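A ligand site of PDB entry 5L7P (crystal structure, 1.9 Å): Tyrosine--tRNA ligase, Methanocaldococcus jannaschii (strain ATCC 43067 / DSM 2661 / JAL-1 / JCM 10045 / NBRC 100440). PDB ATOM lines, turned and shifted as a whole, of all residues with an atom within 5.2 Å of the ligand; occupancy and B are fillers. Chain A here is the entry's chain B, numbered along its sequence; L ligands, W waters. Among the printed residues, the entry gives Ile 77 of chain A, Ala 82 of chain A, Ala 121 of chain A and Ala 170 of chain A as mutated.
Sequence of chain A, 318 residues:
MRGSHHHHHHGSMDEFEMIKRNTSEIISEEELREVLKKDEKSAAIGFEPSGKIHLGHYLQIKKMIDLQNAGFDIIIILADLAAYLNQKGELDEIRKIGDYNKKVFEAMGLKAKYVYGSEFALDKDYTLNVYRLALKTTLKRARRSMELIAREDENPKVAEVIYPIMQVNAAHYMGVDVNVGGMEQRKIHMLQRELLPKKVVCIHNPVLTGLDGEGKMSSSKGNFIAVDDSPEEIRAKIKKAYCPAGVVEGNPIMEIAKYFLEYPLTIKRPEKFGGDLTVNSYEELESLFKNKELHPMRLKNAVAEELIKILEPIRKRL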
ATOM      1  N   ILE A  45      15.121  15.398  -3.214  1.00  0.00           N
ATOM      2  CA  ILE A  45      15.297  14.380  -4.231  1.00  0.00           C
ATOM      3  C   ILE A  45      16.741  13.911  -4.149  1.00  0.00           C
ATOM      4  O   ILE A  45      17.646  14.685  -3.828  1.00  0.00           O
ATOM      5  CB  ILE A  45      15.002  14.873  -5.661  1.00  0.00           C
ATOM      6  CG1 ILE A  45      15.144  13.730  -6.658  1.00  0.00           C
ATOM      7  CG2 ILE A  45      15.914  15.993  -6.025  1.00  0.00           C
ATOM      8  CD1 ILE A  45      14.367  13.989  -7.981  1.00  0.00           C
ATOM      9  N   GLY A  46      16.955  12.634  -4.443  1.00  0.00           N
ATOM     10  CA  GLY A  46      18.305  12.078  -4.518  1.00  0.00           C
ATOM     11  C   GLY A  46      18.673  11.589  -5.925  1.00  0.00           C
ATOM     12  O   GLY A  46      17.839  11.001  -6.604  1.00  0.00           O
ATOM     13  N   PHE A  47      19.934  11.760  -6.286  1.00  0.00           N
ATOM     14  CA  PHE A  47      20.429  11.237  -7.547  1.00  0.00           C
ATOM     15  C   PHE A  47      21.722  10.462  -7.320  1.00  0.00           C
ATOM     16  O   PHE A  47      22.681  11.041  -6.829  1.00  0.00           O
ATOM     17  CB  PHE A  47      20.762  12.368  -8.527  1.00  0.00           C
ATOM     18  CG  PHE A  47      19.602  13.255  -8.897  1.00  0.00           C
ATOM     19  CD1 PHE A  47      18.728  12.887  -9.928  1.00  0.00           C
ATOM     20  CD2 PHE A  47      19.430  14.488  -8.283  1.00  0.00           C
ATOM     21  CE1 PHE A  47      17.669  13.720 -10.279  1.00  0.00           C
ATOM     22  CE2 PHE A  47      18.371  15.307  -8.637  1.00  0.00           C
ATOM     23  CZ  PHE A  47      17.512  14.929  -9.643  1.00  0.00           C
ATOM     24  N   GLU A  48      21.784   9.194  -7.781  1.00  0.00           N
ATOM     25  CA  GLU A  48      23.088   8.548  -7.918  1.00  0.00           C
ATOM     26  C   GLU A  48      23.941   9.385  -8.866  1.00  0.00           C
ATOM     27  O   GLU A  48      23.489   9.664  -9.978  1.00  0.00           O
ATOM     28  CB  GLU A  48      22.973   7.122  -8.458  1.00  0.00           C
ATOM     29  CG  GLU A  48      22.266   6.162  -7.501  1.00  0.00           C
ATOM     30  CD  GLU A  48      22.253   4.738  -8.012  1.00  0.00           C
ATOM     31  OE1 GLU A  48      23.218   4.347  -8.684  1.00  0.00           O
ATOM     32  OE2 GLU A  48      21.279   4.017  -7.752  1.00  0.00           O
ATOM     33  N   ILE A  77      20.124  15.456  -2.736  1.00  0.00           N
ATOM     34  CA  ILE A  77      21.097  14.488  -2.233  1.00  0.00           C
ATOM     35  C   ILE A  77      21.953  13.996  -3.386  1.00  0.00           C
ATOM     36  O   ILE A  77      21.452  13.367  -4.325  1.00  0.00           O
ATOM     37  CB  ILE A  77      20.387  13.310  -1.547  1.00  0.00           C
ATOM     38  CG1 ILE A  77      19.576  13.846  -0.363  1.00  0.00           C
ATOM     39  CG2 ILE A  77      21.426  12.219  -1.121  1.00  0.00           C
ATOM     40  CD1 ILE A  77      18.555  12.886   0.157  1.00  0.00           C
ATOM     41  N   LEU A  78      23.248  14.262  -3.320  1.00  0.00           N
ATOM     42  CA  LEU A  78      24.208  13.655  -4.232  1.00  0.00           C
ATOM     43  C   LEU A  78      24.512  12.275  -3.665  1.00  0.00           C
ATOM     44  O   LEU A  78      25.295  12.140  -2.718  1.00  0.00           O
ATOM     45  CB  LEU A  78      25.444  14.536  -4.347  1.00  0.00           C
ATOM     46  CG  LEU A  78      25.135  15.989  -4.797  1.00  0.00           C
ATOM     47  CD1 LEU A  78      26.357  16.877  -4.672  1.00  0.00           C
ATOM     48  CD2 LEU A  78      24.635  15.973  -6.270  1.00  0.00           C
ATOM     49  N   ALA A  79      23.853  11.234  -4.185  1.00  0.00           N
ATOM     50  CA  ALA A  79      23.726   9.974  -3.444  1.00  0.00           C
ATOM     51  C   ALA A  79      24.940   9.070  -3.704  1.00  0.00           C
ATOM     52  O   ALA A  79      24.847   8.001  -4.312  1.00  0.00           O
ATOM     53  CB  ALA A  79      22.420   9.276  -3.791  1.00  0.00           C
ATOM     54  N   ASP A  80      26.082   9.472  -3.109  1.00  0.00           N
ATOM     55  CA  ASP A  80      27.334   8.742  -3.338  1.00  0.00           C
ATOM     56  C   ASP A  80      27.278   7.344  -2.750  1.00  0.00           C
ATOM     57  O   ASP A  80      27.728   6.369  -3.366  1.00  0.00           O
ATOM     58  CB  ASP A  80      28.559   9.519  -2.790  1.00  0.00           C
ATOM     59  CG  ASP A  80      28.471   9.864  -1.308  1.00  0.00           C
ATOM     60  OD1 ASP A  80      27.380   9.964  -0.735  1.00  0.00           O
ATOM     61  OD2 ASP A  80      29.542  10.105  -0.698  1.00  0.00           O
ATOM     62  N   LEU A  81      26.693   7.186  -1.583  1.00  0.00           N
ATOM     63  CA  LEU A  81      26.640   5.859  -0.991  1.00  0.00           C
ATOM     64  C   LEU A  81      25.623   4.961  -1.703  1.00  0.00           C
ATOM     65  O   LEU A  81      25.865   3.762  -1.870  1.00  0.00           O
ATOM     66  CB  LEU A  81      26.310   6.020   0.483  1.00  0.00           C
ATOM     67  CG  LEU A  81      26.756   5.046   1.543  1.00  0.00           C
ATOM     68  CD1 LEU A  81      28.125   4.502   1.243  1.00  0.00           C
ATOM     69  CD2 LEU A  81      26.750   5.823   2.861  1.00  0.00           C
ATOM     70  N   ALA A  82      24.491   5.511  -2.158  1.00  0.00           N
ATOM     71  CA  ALA A  82      23.588   4.711  -2.978  1.00  0.00           C
ATOM     72  C   ALA A  82      24.277   4.232  -4.239  1.00  0.00           C
ATOM     73  O   ALA A  82      24.170   3.073  -4.624  1.00  0.00           O
ATOM     74  CB  ALA A  82      22.336   5.512  -3.348  1.00  0.00           C
ATOM     75  N   LEU A  85      26.622   1.388  -3.303  1.00  0.00           N
ATOM     76  CA  LEU A  85      25.877   0.152  -3.091  1.00  0.00           C
ATOM     77  C   LEU A  85      25.347  -0.425  -4.399  1.00  0.00           C
ATOM     78  O   LEU A  85      25.195  -1.645  -4.522  1.00  0.00           O
ATOM     79  CB  LEU A  85      24.727   0.368  -2.123  1.00  0.00           C
ATOM     80  CG  LEU A  85      25.117   0.595  -0.665  1.00  0.00           C
ATOM     81  CD1 LEU A  85      23.936   1.123   0.129  1.00  0.00           C
ATOM     82  CD2 LEU A  85      25.629  -0.665  -0.007  1.00  0.00           C
ATOM     83  N   GLY A 117      25.091  11.976   0.327  1.00  0.00           N
ATOM     84  CA  GLY A 117      24.401  11.038   1.198  1.00  0.00           C
ATOM     85  C   GLY A 117      25.270  10.647   2.375  1.00  0.00           C
ATOM     86  O   GLY A 117      24.793  10.601   3.519  1.00  0.00           O
ATOM     87  N   SER A 118      26.561  10.431   2.122  1.00  0.00           N
ATOM     88  CA  SER A 118      27.510  10.004   3.137  1.00  0.00           C
ATOM     89  C   SER A 118      27.744  11.027   4.240  1.00  0.00           C
ATOM     90  O   SER A 118      28.357  10.686   5.260  1.00  0.00           O
ATOM     91  CB  SER A 118      28.835   9.661   2.470  1.00  0.00           C
ATOM     92  OG  SER A 118      29.372  10.760   1.785  1.00  0.00           O
ATOM     93  N   PHE A 120      25.338  12.223   6.008  1.00  0.00           N
ATOM     94  CA  PHE A 120      24.389  11.866   7.047  1.00  0.00           C
ATOM     95  C   PHE A 120      24.068  10.382   7.113  1.00  0.00           C
ATOM     96  O   PHE A 120      23.712   9.909   8.193  1.00  0.00           O
ATOM     97  CB  PHE A 120      23.073  12.653   6.878  1.00  0.00           C
ATOM     98  CG  PHE A 120      22.380  12.404   5.583  1.00  0.00           C
ATOM     99  CD1 PHE A 120      21.470  11.395   5.451  1.00  0.00           C
ATOM    100  CD2 PHE A 120      22.662  13.189   4.485  1.00  0.00           C
ATOM    101  CE1 PHE A 120      20.833  11.166   4.249  1.00  0.00           C
ATOM    102  CE2 PHE A 120      22.033  12.967   3.286  1.00  0.00           C
ATOM    103  CZ  PHE A 120      21.110  11.947   3.170  1.00  0.00           C
ATOM    104  N   ALA A 121      24.248   9.624   6.048  1.00  0.00           N
ATOM    105  CA  ALA A 121      23.710   8.272   6.023  1.00  0.00           C
ATOM    106  C   ALA A 121      24.622   7.291   6.718  1.00  0.00           C
ATOM    107  O   ALA A 121      24.327   6.086   6.714  1.00  0.00           O
ATOM    108  CB  ALA A 121      23.423   7.855   4.581  1.00  0.00           C
ATOM    109  N   TYR A 126      21.252   7.149  12.160  1.00  0.00           N
ATOM    110  CA  TYR A 126      20.737   6.751  10.857  1.00  0.00           C
ATOM    111  C   TYR A 126      20.858   5.246  10.676  1.00  0.00           C
ATOM    112  O   TYR A 126      19.883   4.560  10.383  1.00  0.00           O
ATOM    113  CB  TYR A 126      21.539   7.474   9.779  1.00  0.00           C
ATOM    114  CG  TYR A 126      20.913   7.460   8.419  1.00  0.00           C
ATOM    115  CD1 TYR A 126      21.005   6.352   7.583  1.00  0.00           C
ATOM    116  CD2 TYR A 126      20.275   8.579   7.953  1.00  0.00           C
ATOM    117  CE1 TYR A 126      20.422   6.372   6.314  1.00  0.00           C
ATOM    118  CE2 TYR A 126      19.711   8.606   6.722  1.00  0.00           C
ATOM    119  CZ  TYR A 126      19.768   7.508   5.910  1.00  0.00           C
ATOM    120  OH  TYR A 126      19.172   7.615   4.674  1.00  0.00           O
ATOM    121  N   ILE A 149      15.746  -0.059 -10.573  1.00  0.00           N
ATOM    122  CA  ILE A 149      16.843   0.757 -10.085  1.00  0.00           C
ATOM    123  C   ILE A 149      18.153  -0.006 -10.051  1.00  0.00           C
ATOM    124  O   ILE A 149      19.218   0.533 -10.381  1.00  0.00           O
ATOM    125  CB  ILE A 149      16.505   1.288  -8.673  1.00  0.00           C
ATOM    126  CG1 ILE A 149      15.222   2.141  -8.736  1.00  0.00           C
ATOM    127  CG2 ILE A 149      17.723   1.992  -8.087  1.00  0.00           C
ATOM    128  CD1 ILE A 149      14.651   2.486  -7.445  1.00  0.00           C
ATOM    129  N   TYR A 163      20.058  -1.005   0.011  1.00  0.00           N
ATOM    130  CA  TYR A 163      19.792   0.265  -0.660  1.00  0.00           C
ATOM    131  C   TYR A 163      18.396   0.806  -0.420  1.00  0.00           C
ATOM    132  O   TYR A 163      18.273   1.962   0.025  1.00  0.00           O
ATOM    133  CB  TYR A 163      20.099   0.041  -2.142  1.00  0.00           C
ATOM    134  CG  TYR A 163      19.931   1.213  -3.108  1.00  0.00           C
ATOM    135  CD1 TYR A 163      18.705   1.824  -3.262  1.00  0.00           C
ATOM    136  CD2 TYR A 163      20.989   1.607  -3.951  1.00  0.00           C
ATOM    137  CE1 TYR A 163      18.524   2.862  -4.204  1.00  0.00           C
ATOM    138  CE2 TYR A 163      20.834   2.654  -4.905  1.00  0.00           C
ATOM    139  CZ  TYR A 163      19.574   3.265  -5.016  1.00  0.00           C
ATOM    140  OH  TYR A 163      19.348   4.263  -5.935  1.00  0.00           O
ATOM    141  N   MET A 166      17.916   2.140   3.130  1.00  0.00           N
ATOM    142  CA  MET A 166      18.608   3.380   3.379  1.00  0.00           C
ATOM    143  C   MET A 166      17.834   4.538   2.776  1.00  0.00           C
ATOM    144  O   MET A 166      17.765   5.619   3.360  1.00  0.00           O
ATOM    145  CB  MET A 166      20.007   3.279   2.808  1.00  0.00           C
ATOM    146  CG  MET A 166      20.873   2.378   3.662  1.00  0.00           C
ATOM    147  SD  MET A 166      22.489   2.372   2.958  1.00  0.00           S
ATOM    148  CE  MET A 166      23.101   3.965   3.563  1.00  0.00           C
ATOM    149  N   GLN A 167      17.195   4.312   1.637  1.00  0.00           N
ATOM    150  CA  GLN A 167      16.453   5.402   1.010  1.00  0.00           C
ATOM    151  C   GLN A 167      15.203   5.743   1.803  1.00  0.00           C
ATOM    152  O   GLN A 167      14.882   6.925   1.987  1.00  0.00           O
ATOM    153  CB  GLN A 167      16.100   5.048  -0.419  1.00  0.00           C
ATOM    154  CG  GLN A 167      15.402   6.201  -1.117  1.00  0.00           C
ATOM    155  CD  GLN A 167      15.365   6.041  -2.590  1.00  0.00           C
ATOM    156  OE1 GLN A 167      16.238   5.381  -3.167  1.00  0.00           O
ATOM    157  NE2 GLN A 167      14.360   6.625  -3.234  1.00  0.00           N
ATOM    158  N   ALA A 170      16.059   8.064   4.601  1.00  0.00           N
ATOM    159  CA  ALA A 170      16.604   9.398   4.329  1.00  0.00           C
ATOM    160  C   ALA A 170      15.564  10.467   4.626  1.00  0.00           C
ATOM    161  O   ALA A 170      15.865  11.484   5.241  1.00  0.00           O
ATOM    162  CB  ALA A 170      17.103   9.520   2.878  1.00  0.00           C
ATOM    163  N   GLU A 184      10.118   5.330 -11.299  1.00  0.00           N
ATOM    164  CA  GLU A 184      10.818   4.112 -10.918  1.00  0.00           C
ATOM    165  C   GLU A 184      11.094   4.044  -9.418  1.00  0.00           C
ATOM    166  O   GLU A 184      11.376   2.954  -8.910  1.00  0.00           O
ATOM    167  CB  GLU A 184      12.107   3.997 -11.733  1.00  0.00           C
ATOM    168  CG  GLU A 184      13.305   4.793 -11.294  1.00  0.00           C
ATOM    169  CD  GLU A 184      13.216   6.288 -11.580  1.00  0.00           C
ATOM    170  OE1 GLU A 184      14.052   7.023 -10.959  1.00  0.00           O
ATOM    171  OE2 GLU A 184      12.341   6.703 -12.407  1.00  0.00           O
ATOM    172  N   GLN A 185      10.963   5.174  -8.705  1.00  0.00           N
ATOM    173  CA  GLN A 185      11.131   5.207  -7.249  1.00  0.00           C
ATOM    174  C   GLN A 185       9.840   4.863  -6.515  1.00  0.00           C
ATOM    175  O   GLN A 185       9.837   4.814  -5.281  1.00  0.00           O
ATOM    176  CB  GLN A 185      11.584   6.599  -6.798  1.00  0.00           C
ATOM    177  CG  GLN A 185      12.741   7.212  -7.584  1.00  0.00           C
ATOM    178  CD  GLN A 185      14.025   6.408  -7.438  1.00  0.00           C
ATOM    179  OE1 GLN A 185      14.352   5.930  -6.334  1.00  0.00           O
ATOM    180  NE2 GLN A 185      14.768   6.266  -8.540  1.00  0.00           N
ATOM    181  N   ILE A 188       9.760   2.085  -3.681  1.00  0.00           N
ATOM    182  CA  ILE A 188      10.450   2.504  -2.451  1.00  0.00           C
ATOM    183  C   ILE A 188       9.581   3.498  -1.697  1.00  0.00           C
ATOM    184  O   ILE A 188       9.448   3.436  -0.470  1.00  0.00           O
ATOM    185  CB  ILE A 188      11.843   3.089  -2.764  1.00  0.00           C
ATOM    186  CG1 ILE A 188      12.805   1.987  -3.237  1.00  0.00           C
ATOM    187  CG2 ILE A 188      12.428   3.778  -1.558  1.00  0.00           C
ATOM    188  CD1 ILE A 188      14.165   2.499  -3.741  1.00  0.00           C
HETATM  189  O1  LIG L   1      19.156   7.763  -8.232  1.00  0.00           O
HETATM  190  C1  LIG L   1      18.283   6.978  -7.734  1.00  0.00           C
HETATM  191  O2  LIG L   1      17.804   5.989  -8.341  1.00  0.00           O
HETATM  192  C2  LIG L   1      17.737   7.244  -6.365  1.00  0.00           C
HETATM  193  N1  LIG L   1      17.206   6.003  -5.808  1.00  0.00           N
HETATM  194  C3  LIG L   1      18.795   7.776  -5.411  1.00  0.00           C
HETATM  195  C4  LIG L   1      18.255   8.342  -4.113  1.00  0.00           C
HETATM  196  C5  LIG L   1      16.946   8.813  -3.883  1.00  0.00           C
HETATM  197  C6  LIG L   1      16.591   9.328  -2.626  1.00  0.00           C
HETATM  198  C7  LIG L   1      17.567   9.405  -1.619  1.00  0.00           C
HETATM  199  O3  LIG L   1      17.195   9.901  -0.413  1.00  0.00           O
HETATM  200  C8  LIG L   1      19.191   8.424  -3.095  1.00  0.00           C
HETATM  201  C9  LIG L   1      18.869   8.928  -1.853  1.00  0.00           C
HETATM  202  O4  LIG L   1      19.916   8.992  -0.975  1.00  0.00           O
HETATM  203  C10 LIG L   1      20.031   8.269   0.215  1.00  0.00           C
HETATM  204  C11 LIG L   1      20.524   6.845  -0.026  1.00  0.00           C
HETATM  205  C12 LIG L   1      21.862   6.476   0.139  1.00  0.00           C
HETATM  206  N2  LIG L   1      22.878   7.420   0.437  1.00  0.00           N
HETATM  207  O5  LIG L   1      23.420   8.093  -0.481  1.00  0.00           O
HETATM  208  O6  LIG L   1      23.235   7.536   1.592  1.00  0.00           O
HETATM  209  C13 LIG L   1      19.581   5.883  -0.381  1.00  0.00           C
HETATM  210  C14 LIG L   1      19.959   4.561  -0.584  1.00  0.00           C
HETATM  211  C15 LIG L   1      21.284   4.193  -0.422  1.00  0.00           C
HETATM  212  C16 LIG L   1      22.230   5.146  -0.058  1.00  0.00           C
HETATM  213  O   HOH W   1      14.260  10.818  -4.507  1.00  0.00           O
HETATM  214  O   HOH W   2      13.180   9.388  -2.410  1.00  0.00           O
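The backbone NH (N) of Ala 82 sits close to an oxygen (O5) of the ligand. N of Glu 48 is in hydrogen-bond range of O1 of the ligand (3.0 Å). N1 of the ligand lies within hydrogen-bond range of OE1 of Gln 185 (2.9 Å). The side-chain amide oxygen (OE1) of Gln 167 is in hydrogen-bond range of a nitrogen (N1) of the ligand (2.9 Å). The side-chain hydroxyl (OH) of Tyr 163 sits at hydrogen-bond distance from a nitrogen (N1) of the ligand.
The backbone NH (N) of Ile 77 lies within hydrogen-bond range of the backbone carbonyl oxygen (O) of Ile 45 (2.8 Å). OG of Ser 118 lies within hydrogen-bond range of OD2 of Asp 80 (2.6 Å). O of Ile 77 sits at hydrogen-bond distance from N of Phe 47 (3.0 Å). The backbone NH of Gly 117 sits at hydrogen-bond distance from the backbone carbonyl oxygen of Leu 78, 3.1 Å away. The side-chain hydroxyl of Tyr 126 is in hydrogen-bond range of the backbone carbonyl oxygen of Met 166, at 2.8 Å. NE2 of Gln 167 sits at hydrogen-bond distance from OE1 of Gln 185 (3.2 Å). O of Phe 47 lies within hydrogen-bond range of N of Ala 79, at 2.9 Å. N of Ala 170 sits close to OH of Tyr 126.
O of Gly 46 touches C3 of the ligand, at 3.6 Å. Phe 47 touches the ligand. Ile 77 touches the ligand (CD1 to O3, 3.3 Å). CB of Ala 79 touches C8 of the ligand, 3.4 Å away. Asp 80 touches the ligand. N of Leu 81 touches O5 of the ligand (3.6 Å). CA of Gly 117 touches O5 of the ligand, at 3.5 Å. Ala 121 touches the ligand. Met 166 touches the ligand. Ala 170 touches the ligand (CB to O3, 3.3 Å). Hydrophobic or aromatic side chains within 4 Å of the ligand: Ile 77, Ala 79, Leu 81, Ala 82, Ala 121, Tyr 163, Met 166 and Ala 170. Of the 24 residues printed, 15 come within 4 Å of the ligand.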
